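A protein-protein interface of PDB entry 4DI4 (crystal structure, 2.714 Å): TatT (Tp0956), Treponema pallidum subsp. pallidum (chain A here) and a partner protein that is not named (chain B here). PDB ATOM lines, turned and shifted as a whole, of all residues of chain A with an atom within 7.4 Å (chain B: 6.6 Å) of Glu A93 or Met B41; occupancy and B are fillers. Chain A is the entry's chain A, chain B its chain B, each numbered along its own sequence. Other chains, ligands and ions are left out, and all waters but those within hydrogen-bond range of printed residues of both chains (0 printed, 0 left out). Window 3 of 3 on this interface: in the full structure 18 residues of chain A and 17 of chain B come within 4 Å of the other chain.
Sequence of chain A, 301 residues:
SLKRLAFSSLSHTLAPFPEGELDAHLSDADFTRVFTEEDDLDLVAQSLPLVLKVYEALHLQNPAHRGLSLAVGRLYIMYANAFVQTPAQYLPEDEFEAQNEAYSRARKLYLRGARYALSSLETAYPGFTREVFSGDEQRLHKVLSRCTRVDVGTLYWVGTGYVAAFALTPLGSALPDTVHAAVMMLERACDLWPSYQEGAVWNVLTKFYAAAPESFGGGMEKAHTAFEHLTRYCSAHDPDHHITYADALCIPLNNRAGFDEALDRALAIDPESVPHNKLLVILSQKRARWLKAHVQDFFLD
NZ of Lys B42 lies within salt-bridge range of OD2 of Asp A297 (3.1 Å).
The side-chain carboxylate of Glu A93 lies close to the backbone carbonyl oxygen of Met B41 (3.4 Å).
OG of Ser B28 lies within hydrogen-bond range of N of Met B41 (3.2 Å).
The backbone NH of Ile B10 is in hydrogen-bond range of the backbone carbonyl oxygen of Lys B42, at 3.1 Å.
The backbone carbonyl oxygen (O) of Leu B8 is in hydrogen-bond range of the backbone NH (N) of Lys B42 (2.8 Å).
Among the printed residues, merely in contact across the chains: Phe A96 with Lys B26, Glu A93 with Lys B25, Asp A94 with Ala B29 and Glu A93 with Lys B42.
Glu A93 touches just these residues of chain B: Lys B25 (3.5 Å), Met B41 (3.4 Å) and Lys B42 (3.8 Å).
Met B41 touches one residue of chain A.
Of the printed residues of chain A, Lys B42 touches Glu A93 (3.8 Å) and Asp A297 (3.1 Å).
Printed residues of chain A within 4 Å of Ala B29: Asp A94 (3.7 Å).
Of the printed residues of chain A, Lys B25 touches Glu A93.
The nearest printed residue of chain B that does not touch Glu A93 is Phe B43 (4.2 Å).
Printed residues of chain B that touch a printed residue of chain A: Lys B25, Lys B26, Ala B29, Met B41 and Lys B42.
Hydrophobic or aromatic side chains of chain B within 4 Å of the printed part of chain A: Ala B29.
Of the 10 printed residues of chain A, 4 touch a printed residue of chain B.
Hydrophobic or aromatic side chains of chain A within 4 Å of the printed part of chain B: Phe A96.
Among the printed residues, 6 pairs touch across the chains.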
ATOM      1  N   TYR A  90      15.818   5.578  18.809  1.00  0.00           N
ATOM      2  CA  TYR A  90      17.184   5.389  19.285  1.00  0.00           C
ATOM      3  C   TYR A  90      17.992   4.565  18.302  1.00  0.00           C
ATOM      4  O   TYR A  90      19.119   4.185  18.592  1.00  0.00           O
ATOM      5  CB  TYR A  90      17.191   4.681  20.651  1.00  0.00           C
ATOM      6  CG  TYR A  90      16.549   5.466  21.770  1.00  0.00           C
ATOM      7  CD1 TYR A  90      16.590   6.854  21.791  1.00  0.00           C
ATOM      8  CD2 TYR A  90      15.903   4.821  22.806  1.00  0.00           C
ATOM      9  CE1 TYR A  90      15.993   7.578  22.817  1.00  0.00           C
ATOM     10  CE2 TYR A  90      15.310   5.532  23.843  1.00  0.00           C
ATOM     11  CZ  TYR A  90      15.351   6.907  23.845  1.00  0.00           C
ATOM     12  OH  TYR A  90      14.758   7.615  24.872  1.00  0.00           O
ATOM     13  N   LEU A  91      17.399   4.237  17.162  1.00  0.00           N
ATOM     14  CA  LEU A  91      18.123   3.518  16.124  1.00  0.00           C
ATOM     15  C   LEU A  91      19.120   4.430  15.422  1.00  0.00           C
ATOM     16  O   LEU A  91      18.875   5.638  15.275  1.00  0.00           O
ATOM     17  CB  LEU A  91      17.160   2.952  15.095  1.00  0.00           C
ATOM     18  CG  LEU A  91      16.325   1.758  15.516  1.00  0.00           C
ATOM     19  CD1 LEU A  91      15.248   1.539  14.479  1.00  0.00           C
ATOM     20  CD2 LEU A  91      17.196   0.518  15.694  1.00  0.00           C
ATOM     21  N   PRO A  92      20.250   3.851  14.986  1.00  0.00           N
ATOM     22  CA  PRO A  92      21.303   4.557  14.226  1.00  0.00           C
ATOM     23  C   PRO A  92      20.768   5.019  12.877  1.00  0.00           C
ATOM     24  O   PRO A  92      19.982   4.286  12.273  1.00  0.00           O
ATOM     25  CB  PRO A  92      22.388   3.483  14.017  1.00  0.00           C
ATOM     26  CG  PRO A  92      22.065   2.369  15.001  1.00  0.00           C
ATOM     27  CD  PRO A  92      20.566   2.428  15.212  1.00  0.00           C
ATOM     28  N   GLU A  93      21.211   6.176  12.393  1.00  0.00           N
ATOM     29  CA  GLU A  93      20.568   6.819  11.248  1.00  0.00           C
ATOM     30  C   GLU A  93      20.631   6.041   9.921  1.00  0.00           C
ATOM     31  O   GLU A  93      20.020   6.444   8.932  1.00  0.00           O
ATOM     32  CB  GLU A  93      21.069   8.260  11.070  1.00  0.00           C
ATOM     33  CG  GLU A  93      19.960   9.241  10.687  1.00  0.00           C
ATOM     34  CD  GLU A  93      20.462  10.397   9.841  1.00  0.00           C
ATOM     35  OE1 GLU A  93      21.276  11.200  10.349  1.00  0.00           O
ATOM     36  OE2 GLU A  93      20.044  10.497   8.664  1.00  0.00           O
ATOM     37  N   ASP A  94      21.392   4.955   9.895  1.00  0.00           N
ATOM     38  CA  ASP A  94      21.421   4.036   8.755  1.00  0.00           C
ATOM     39  C   ASP A  94      20.459   2.851   8.904  1.00  0.00           C
ATOM     40  O   ASP A  94      20.203   2.114   7.959  1.00  0.00           O
ATOM     41  CB  ASP A  94      22.838   3.516   8.608  1.00  0.00           C
ATOM     42  CG  ASP A  94      23.477   3.275   9.947  1.00  0.00           C
ATOM     43  OD1 ASP A  94      23.633   2.095  10.317  1.00  0.00           O
ATOM     44  OD2 ASP A  94      23.770   4.272  10.650  1.00  0.00           O
ATOM     45  N   GLU A  95      19.910   2.691  10.098  1.00  0.00           N
ATOM     46  CA  GLU A  95      18.944   1.651  10.366  1.00  0.00           C
ATOM     47  C   GLU A  95      17.571   2.206  10.026  1.00  0.00           C
ATOM     48  O   GLU A  95      16.541   1.627  10.366  1.00  0.00           O
ATOM     49  CB  GLU A  95      19.009   1.215  11.829  1.00  0.00           C
ATOM     50  CG  GLU A  95      18.614  -0.234  12.017  1.00  0.00           C
ATOM     51  CD  GLU A  95      19.328  -1.119  11.021  1.00  0.00           C
ATOM     52  OE1 GLU A  95      20.569  -1.010  10.964  1.00  0.00           O
ATOM     53  OE2 GLU A  95      18.659  -1.893  10.293  1.00  0.00           O
ATOM     54  N   PHE A  96      17.571   3.370   9.390  1.00  0.00           N
ATOM     55  CA  PHE A  96      16.356   4.112   9.112  1.00  0.00           C
ATOM     56  C   PHE A  96      15.239   3.317   8.407  1.00  0.00           C
ATOM     57  O   PHE A  96      14.074   3.698   8.496  1.00  0.00           O
ATOM     58  CB  PHE A  96      16.692   5.358   8.297  1.00  0.00           C
ATOM     59  CG  PHE A  96      16.819   5.096   6.834  1.00  0.00           C
ATOM     60  CD1 PHE A  96      15.852   5.552   5.954  1.00  0.00           C
ATOM     61  CD2 PHE A  96      17.894   4.371   6.337  1.00  0.00           C
ATOM     62  CE1 PHE A  96      15.959   5.302   4.600  1.00  0.00           C
ATOM     63  CE2 PHE A  96      18.009   4.117   4.983  1.00  0.00           C
ATOM     64  CZ  PHE A  96      17.039   4.582   4.113  1.00  0.00           C
ATOM     65  N   GLU A  97      15.570   2.240   7.700  1.00  0.00           N
ATOM     66  CA  GLU A  97      14.515   1.415   7.100  1.00  0.00           C
ATOM     67  C   GLU A  97      13.797   0.621   8.181  1.00  0.00           C
ATOM     68  O   GLU A  97      12.562   0.532   8.202  1.00  0.00           O
ATOM     69  CB  GLU A  97      15.067   0.479   6.030  1.00  0.00           C
ATOM     70  CG  GLU A  97      14.303   0.559   4.722  1.00  0.00           C
ATOM     71  CD  GLU A  97      15.093   0.008   3.545  1.00  0.00           C
ATOM     72  OE1 GLU A  97      15.304  -1.223   3.498  1.00  0.00           O
ATOM     73  OE2 GLU A  97      15.503   0.805   2.667  1.00  0.00           O
ATOM     74  N   GLN A  99      13.841   1.593  11.141  1.00  0.00           N
ATOM     75  CA  GLN A  99      13.179   2.614  11.925  1.00  0.00           C
ATOM     76  C   GLN A  99      11.828   3.004  11.303  1.00  0.00           C
ATOM     77  O   GLN A  99      10.869   3.285  12.022  1.00  0.00           O
ATOM     78  CB  GLN A  99      14.084   3.820  12.123  1.00  0.00           C
ATOM     79  CG  GLN A  99      13.427   4.996  12.839  1.00  0.00           C
ATOM     80  CD  GLN A  99      14.347   6.197  12.903  1.00  0.00           C
ATOM     81  OE1 GLN A  99      14.506   6.929  11.919  1.00  0.00           O
ATOM     82  NE2 GLN A  99      14.982   6.392  14.058  1.00  0.00           N
ATOM     83  N   ASP A 297      23.265  17.846  17.139  1.00  0.00           N
ATOM     84  CA  ASP A 297      22.457  17.614  15.940  1.00  0.00           C
ATOM     85  C   ASP A 297      21.207  18.478  15.853  1.00  0.00           C
ATOM     86  O   ASP A 297      20.594  18.583  14.793  1.00  0.00           O
ATOM     87  CB  ASP A 297      22.054  16.152  15.850  1.00  0.00           C
ATOM     88  CG  ASP A 297      23.213  15.223  16.097  1.00  0.00           C
ATOM     89  OD1 ASP A 297      24.372  15.638  15.855  1.00  0.00           O
ATOM     90  OD2 ASP A 297      22.961  14.081  16.540  1.00  0.00           O
ATOM     91  N   VAL B   6      34.562  12.337   9.276  1.00  0.00           N
ATOM     92  CA  VAL B   6      33.813  13.433   8.665  1.00  0.00           C
ATOM     93  C   VAL B   6      32.283  13.360   8.797  1.00  0.00           C
ATOM     94  O   VAL B   6      31.656  12.352   8.457  1.00  0.00           O
ATOM     95  CB  VAL B   6      34.178  13.573   7.179  1.00  0.00           C
ATOM     96  CG1 VAL B   6      33.150  14.438   6.453  1.00  0.00           C
ATOM     97  CG2 VAL B   6      35.558  14.167   7.029  1.00  0.00           C
ATOM     98  N   VAL B   7      31.694  14.464   9.258  1.00  0.00           N
ATOM     99  CA  VAL B   7      30.242  14.602   9.389  1.00  0.00           C
ATOM    100  C   VAL B   7      29.774  15.947   8.832  1.00  0.00           C
ATOM    101  O   VAL B   7      30.260  17.004   9.238  1.00  0.00           O
ATOM    102  CB  VAL B   7      29.793  14.460  10.858  1.00  0.00           C
ATOM    103  CG1 VAL B   7      28.379  14.979  11.035  1.00  0.00           C
ATOM    104  CG2 VAL B   7      29.914  13.006  11.311  1.00  0.00           C
ATOM    105  N   LEU B   8      28.833  15.901   7.895  1.00  0.00           N
ATOM    106  CA  LEU B   8      28.389  17.104   7.200  1.00  0.00           C
ATOM    107  C   LEU B   8      27.044  17.632   7.683  1.00  0.00           C
ATOM    108  O   LEU B   8      26.077  16.881   7.799  1.00  0.00           O
ATOM    109  CB  LEU B   8      28.300  16.823   5.705  1.00  0.00           C
ATOM    110  CG  LEU B   8      29.611  16.367   5.074  1.00  0.00           C
ATOM    111  CD1 LEU B   8      29.373  15.810   3.687  1.00  0.00           C
ATOM    112  CD2 LEU B   8      30.618  17.513   5.049  1.00  0.00           C
ATOM    113  N   LYS B   9      26.977  18.934   7.937  1.00  0.00           N
ATOM    114  CA  LYS B   9      25.706  19.565   8.265  1.00  0.00           C
ATOM    115  C   LYS B   9      25.047  20.110   7.011  1.00  0.00           C
ATOM    116  O   LYS B   9      25.542  21.055   6.393  1.00  0.00           O
ATOM    117  CB  LYS B   9      25.886  20.714   9.254  1.00  0.00           C
ATOM    118  CG  LYS B   9      27.102  20.611  10.132  1.00  0.00           C
ATOM    119  CD  LYS B   9      27.041  19.441  11.069  1.00  0.00           C
ATOM    120  CE  LYS B   9      27.907  19.745  12.265  1.00  0.00           C
ATOM    121  NZ  LYS B   9      27.621  21.133  12.739  1.00  0.00           N
ATOM    122  N   ILE B  10      23.921  19.512   6.648  1.00  0.00           N
ATOM    123  CA  ILE B  10      23.115  20.021   5.561  1.00  0.00           C
ATOM    124  C   ILE B  10      21.847  20.631   6.126  1.00  0.00           C
ATOM    125  O   ILE B  10      21.006  19.927   6.679  1.00  0.00           O
ATOM    126  CB  ILE B  10      22.711  18.909   4.590  1.00  0.00           C
ATOM    127  CG1 ILE B  10      23.882  17.948   4.343  1.00  0.00           C
ATOM    128  CG2 ILE B  10      22.161  19.505   3.298  1.00  0.00           C
ATOM    129  CD1 ILE B  10      25.189  18.638   4.071  1.00  0.00           C
ATOM    130  N   LEU B  24      16.630  11.786   1.556  1.00  0.00           N
ATOM    131  CA  LEU B  24      17.878  12.401   1.986  1.00  0.00           C
ATOM    132  C   LEU B  24      18.611  11.545   3.003  1.00  0.00           C
ATOM    133  O   LEU B  24      19.822  11.668   3.176  1.00  0.00           O
ATOM    134  CB  LEU B  24      17.621  13.788   2.569  1.00  0.00           C
ATOM    135  CG  LEU B  24      17.172  14.828   1.548  1.00  0.00           C
ATOM    136  CD1 LEU B  24      16.990  16.174   2.232  1.00  0.00           C
ATOM    137  CD2 LEU B  24      18.185  14.904   0.415  1.00  0.00           C
ATOM    138  N   LYS B  25      17.864  10.707   3.705  1.00  0.00           N
ATOM    139  CA  LYS B  25      18.461   9.784   4.652  1.00  0.00           C
ATOM    140  C   LYS B  25      18.979   8.543   3.946  1.00  0.00           C
ATOM    141  O   LYS B  25      20.094   8.088   4.212  1.00  0.00           O
ATOM    142  CB  LYS B  25      17.444   9.433   5.727  1.00  0.00           C
ATOM    143  CG  LYS B  25      16.928  10.673   6.409  1.00  0.00           C
ATOM    144  CD  LYS B  25      16.637  10.408   7.876  1.00  0.00           C
ATOM    145  CE  LYS B  25      15.152  10.237   8.116  1.00  0.00           C
ATOM    146  NZ  LYS B  25      14.709  11.122   9.214  1.00  0.00           N
ATOM    147  N   LYS B  26      18.164   8.022   3.028  1.00  0.00           N
ATOM    148  CA  LYS B  26      18.532   6.867   2.218  1.00  0.00           C
ATOM    149  C   LYS B  26      19.872   7.148   1.527  1.00  0.00           C
ATOM    150  O   LYS B  26      20.688   6.241   1.348  1.00  0.00           O
ATOM    151  CB  LYS B  26      17.425   6.551   1.191  1.00  0.00           C
ATOM    152  CG  LYS B  26      17.402   5.109   0.641  1.00  0.00           C
ATOM    153  CD  LYS B  26      18.650   4.755  -0.180  1.00  0.00           C
ATOM    154  CE  LYS B  26      18.701   3.259  -0.548  1.00  0.00           C
ATOM    155  NZ  LYS B  26      20.048   2.782  -1.036  1.00  0.00           N
ATOM    156  N   LEU B  27      20.093   8.409   1.155  1.00  0.00           N
ATOM    157  CA  LEU B  27      21.350   8.829   0.550  1.00  0.00           C
ATOM    158  C   LEU B  27      22.453   8.904   1.603  1.00  0.00           C
ATOM    159  O   LEU B  27      23.551   8.380   1.393  1.00  0.00           O
ATOM    160  CB  LEU B  27      21.202  10.180  -0.158  1.00  0.00           C
ATOM    161  CG  LEU B  27      22.489  10.665  -0.851  1.00  0.00           C
ATOM    162  CD1 LEU B  27      22.850   9.811  -2.079  1.00  0.00           C
ATOM    163  CD2 LEU B  27      22.419  12.143  -1.232  1.00  0.00           C
ATOM    164  N   SER B  28      22.160   9.552   2.729  1.00  0.00           N
ATOM    165  CA  SER B  28      23.128   9.672   3.820  1.00  0.00           C
ATOM    166  C   SER B  28      23.608   8.313   4.323  1.00  0.00           C
ATOM    167  O   SER B  28      24.768   8.151   4.675  1.00  0.00           O
ATOM    168  CB  SER B  28      22.551  10.480   4.986  1.00  0.00           C
ATOM    169  OG  SER B  28      23.419  10.441   6.112  1.00  0.00           O
ATOM    170  N   ALA B  29      22.709   7.338   4.368  1.00  0.00           N
ATOM    171  CA  ALA B  29      23.100   5.990   4.758  1.00  0.00           C
ATOM    172  C   ALA B  29      23.783   5.258   3.595  1.00  0.00           C
ATOM    173  O   ALA B  29      24.641   4.396   3.806  1.00  0.00           O
ATOM    174  CB  ALA B  29      21.899   5.211   5.263  1.00  0.00           C
ATOM    175  N   TRP B  31      25.663   6.756   1.358  1.00  0.00           N
ATOM    176  CA  TRP B  31      27.016   7.307   1.339  1.00  0.00           C
ATOM    177  C   TRP B  31      27.846   6.731   2.479  1.00  0.00           C
ATOM    178  O   TRP B  31      28.942   6.208   2.263  1.00  0.00           O
ATOM    179  CB  TRP B  31      27.008   8.830   1.491  1.00  0.00           C
ATOM    180  CG  TRP B  31      26.763   9.611   0.245  1.00  0.00           C
ATOM    181  CD1 TRP B  31      26.487   9.123  -0.999  1.00  0.00           C
ATOM    182  CD2 TRP B  31      26.760  11.040   0.127  1.00  0.00           C
ATOM    183  NE1 TRP B  31      26.308  10.163  -1.884  1.00  0.00           N
ATOM    184  CE2 TRP B  31      26.467  11.348  -1.214  1.00  0.00           C
ATOM    185  CE3 TRP B  31      26.967  12.086   1.029  1.00  0.00           C
ATOM    186  CZ2 TRP B  31      26.383  12.661  -1.674  1.00  0.00           C
ATOM    187  CZ3 TRP B  31      26.882  13.386   0.571  1.00  0.00           C
ATOM    188  CH2 TRP B  31      26.598  13.664  -0.766  1.00  0.00           C
ATOM    189  N   SER B  32      27.318   6.841   3.693  1.00  0.00           N
ATOM    190  CA  SER B  32      28.041   6.421   4.884  1.00  0.00           C
ATOM    191  C   SER B  32      28.673   5.059   4.640  1.00  0.00           C
ATOM    192  O   SER B  32      29.895   4.911   4.650  1.00  0.00           O
ATOM    193  CB  SER B  32      27.098   6.352   6.080  1.00  0.00           C
ATOM    194  OG  SER B  32      27.796   5.998   7.253  1.00  0.00           O
ATOM    195  N   VAL B  39      32.216   9.082   6.419  1.00  0.00           N
ATOM    196  CA  VAL B  39      31.503  10.305   6.077  1.00  0.00           C
ATOM    197  C   VAL B  39      29.989  10.125   6.103  1.00  0.00           C
ATOM    198  O   VAL B  39      29.473   9.091   5.683  1.00  0.00           O
ATOM    199  CB  VAL B  39      31.934  10.814   4.697  1.00  0.00           C
ATOM    200  CG1 VAL B  39      31.121  12.031   4.306  1.00  0.00           C
ATOM    201  CG2 VAL B  39      33.418  11.141   4.706  1.00  0.00           C
ATOM    202  N   SER B  40      29.276  11.138   6.593  1.00  0.00           N
ATOM    203  CA  SER B  40      27.813  11.068   6.686  1.00  0.00           C
ATOM    204  C   SER B  40      27.126  12.437   6.678  1.00  0.00           C
ATOM    205  O   SER B  40      27.782  13.476   6.574  1.00  0.00           O
ATOM    206  CB  SER B  40      27.391  10.282   7.927  1.00  0.00           C
ATOM    207  OG  SER B  40      27.943  10.856   9.097  1.00  0.00           O
ATOM    208  N   MET B  41      25.798  12.427   6.791  1.00  0.00           N
ATOM    209  CA  MET B  41      25.009  13.654   6.712  1.00  0.00           C
ATOM    210  C   MET B  41      24.039  13.819   7.876  1.00  0.00           C
ATOM    211  O   MET B  41      23.205  12.955   8.129  1.00  0.00           O
ATOM    212  CB  MET B  41      24.248  13.726   5.383  1.00  0.00           C
ATOM    213  CG  MET B  41      25.063  14.312   4.238  1.00  0.00           C
ATOM    214  SD  MET B  41      24.161  14.428   2.677  1.00  0.00           S
ATOM    215  CE  MET B  41      23.516  12.755   2.567  1.00  0.00           C
ATOM    216  N   LYS B  42      24.161  14.941   8.576  1.00  0.00           N
ATOM    217  CA  LYS B  42      23.236  15.314   9.637  1.00  0.00           C
ATOM    218  C   LYS B  42      22.355  16.476   9.165  1.00  0.00           C
ATOM    219  O   LYS B  42      22.851  17.547   8.852  1.00  0.00           O
ATOM    220  CB  LYS B  42      24.019  15.696  10.900  1.00  0.00           C
ATOM    221  CG  LYS B  42      24.400  14.513  11.791  1.00  0.00           C
ATOM    222  CD  LYS B  42      23.148  13.917  12.459  1.00  0.00           C
ATOM    223  CE  LYS B  42      23.426  12.594  13.173  1.00  0.00           C
ATOM    224  NZ  LYS B  42      24.468  12.728  14.234  1.00  0.00           N
ATOM    225  N   PHE B  43      21.044  16.269   9.114  1.00  0.00           N
ATOM    226  CA  PHE B  43      20.142  17.285   8.565  1.00  0.00           C
ATOM    227  C   PHE B  43      19.597  18.287   9.586  1.00  0.00           C
ATOM    228  O   PHE B  43      19.232  17.918  10.707  1.00  0.00           O
ATOM    229  CB  PHE B  43      19.005  16.622   7.782  1.00  0.00           C
ATOM    230  CG  PHE B  43      19.489  15.758   6.667  1.00  0.00           C
ATOM    231  CD1 PHE B  43      19.616  14.393   6.835  1.00  0.00           C
ATOM    232  CD2 PHE B  43      19.872  16.319   5.458  1.00  0.00           C
ATOM    233  CE1 PHE B  43      20.082  13.595   5.803  1.00  0.00           C
ATOM    234  CE2 PHE B  43      20.338  15.528   4.430  1.00  0.00           C
ATOM    235  CZ  PHE B  43      20.441  14.164   4.599  1.00  0.00           C
ATOM    236  N   ILE B 127      25.453  18.581  -5.660  1.00  0.00           N
ATOM    237  CA  ILE B 127      25.347  17.157  -5.385  1.00  0.00           C
ATOM    238  C   ILE B 127      24.319  16.537  -6.316  1.00  0.00           C
ATOM    239  O   ILE B 127      24.552  15.482  -6.910  1.00  0.00           O
ATOM    240  CB  ILE B 127      24.910  16.917  -3.931  1.00  0.00           C
ATOM    241  CG1 ILE B 127      25.669  17.862  -2.997  1.00  0.00           C
ATOM    242  CG2 ILE B 127      25.089  15.451  -3.538  1.00  0.00           C
ATOM    243  CD1 ILE B 127      27.163  17.737  -3.092  1.00  0.00           C
ATOM    244  N   MET B 226      20.206  20.760  -4.045  1.00  0.00           N
ATOM    245  CA  MET B 226      21.231  20.375  -3.053  1.00  0.00           C
ATOM    246  C   MET B 226      22.690  20.782  -3.351  1.00  0.00           C
ATOM    247  O   MET B 226      23.297  20.316  -4.322  1.00  0.00           O
ATOM    248  CB  MET B 226      21.208  18.883  -2.749  1.00  0.00           C
ATOM    249  CG  MET B 226      22.161  18.507  -1.601  1.00  0.00           C
ATOM    250  SD  MET B 226      22.034  16.792  -1.030  1.00  0.00           S
ATOM    251  CE  MET B 226      23.098  16.807   0.411  1.00  0.00           C
ATOM    252  N   ILE B 228      26.747  21.386  -1.644  1.00  0.00           N
ATOM    253  CA  ILE B 228      27.713  21.243  -0.553  1.00  0.00           C
ATOM    254  C   ILE B 228      28.940  22.151  -0.748  1.00  0.00           C
ATOM    255  O   ILE B 228      29.394  22.362  -1.870  1.00  0.00           O
ATOM    256  CB  ILE B 228      28.177  19.801  -0.406  1.00  0.00           C
ATOM    257  CG1 ILE B 228      28.734  19.581   0.993  1.00  0.00           C
ATOM    258  CG2 ILE B 228      29.241  19.491  -1.433  1.00  0.00           C
ATOM    259  CD1 ILE B 228      29.218  18.184   1.212  1.00  0.00           C
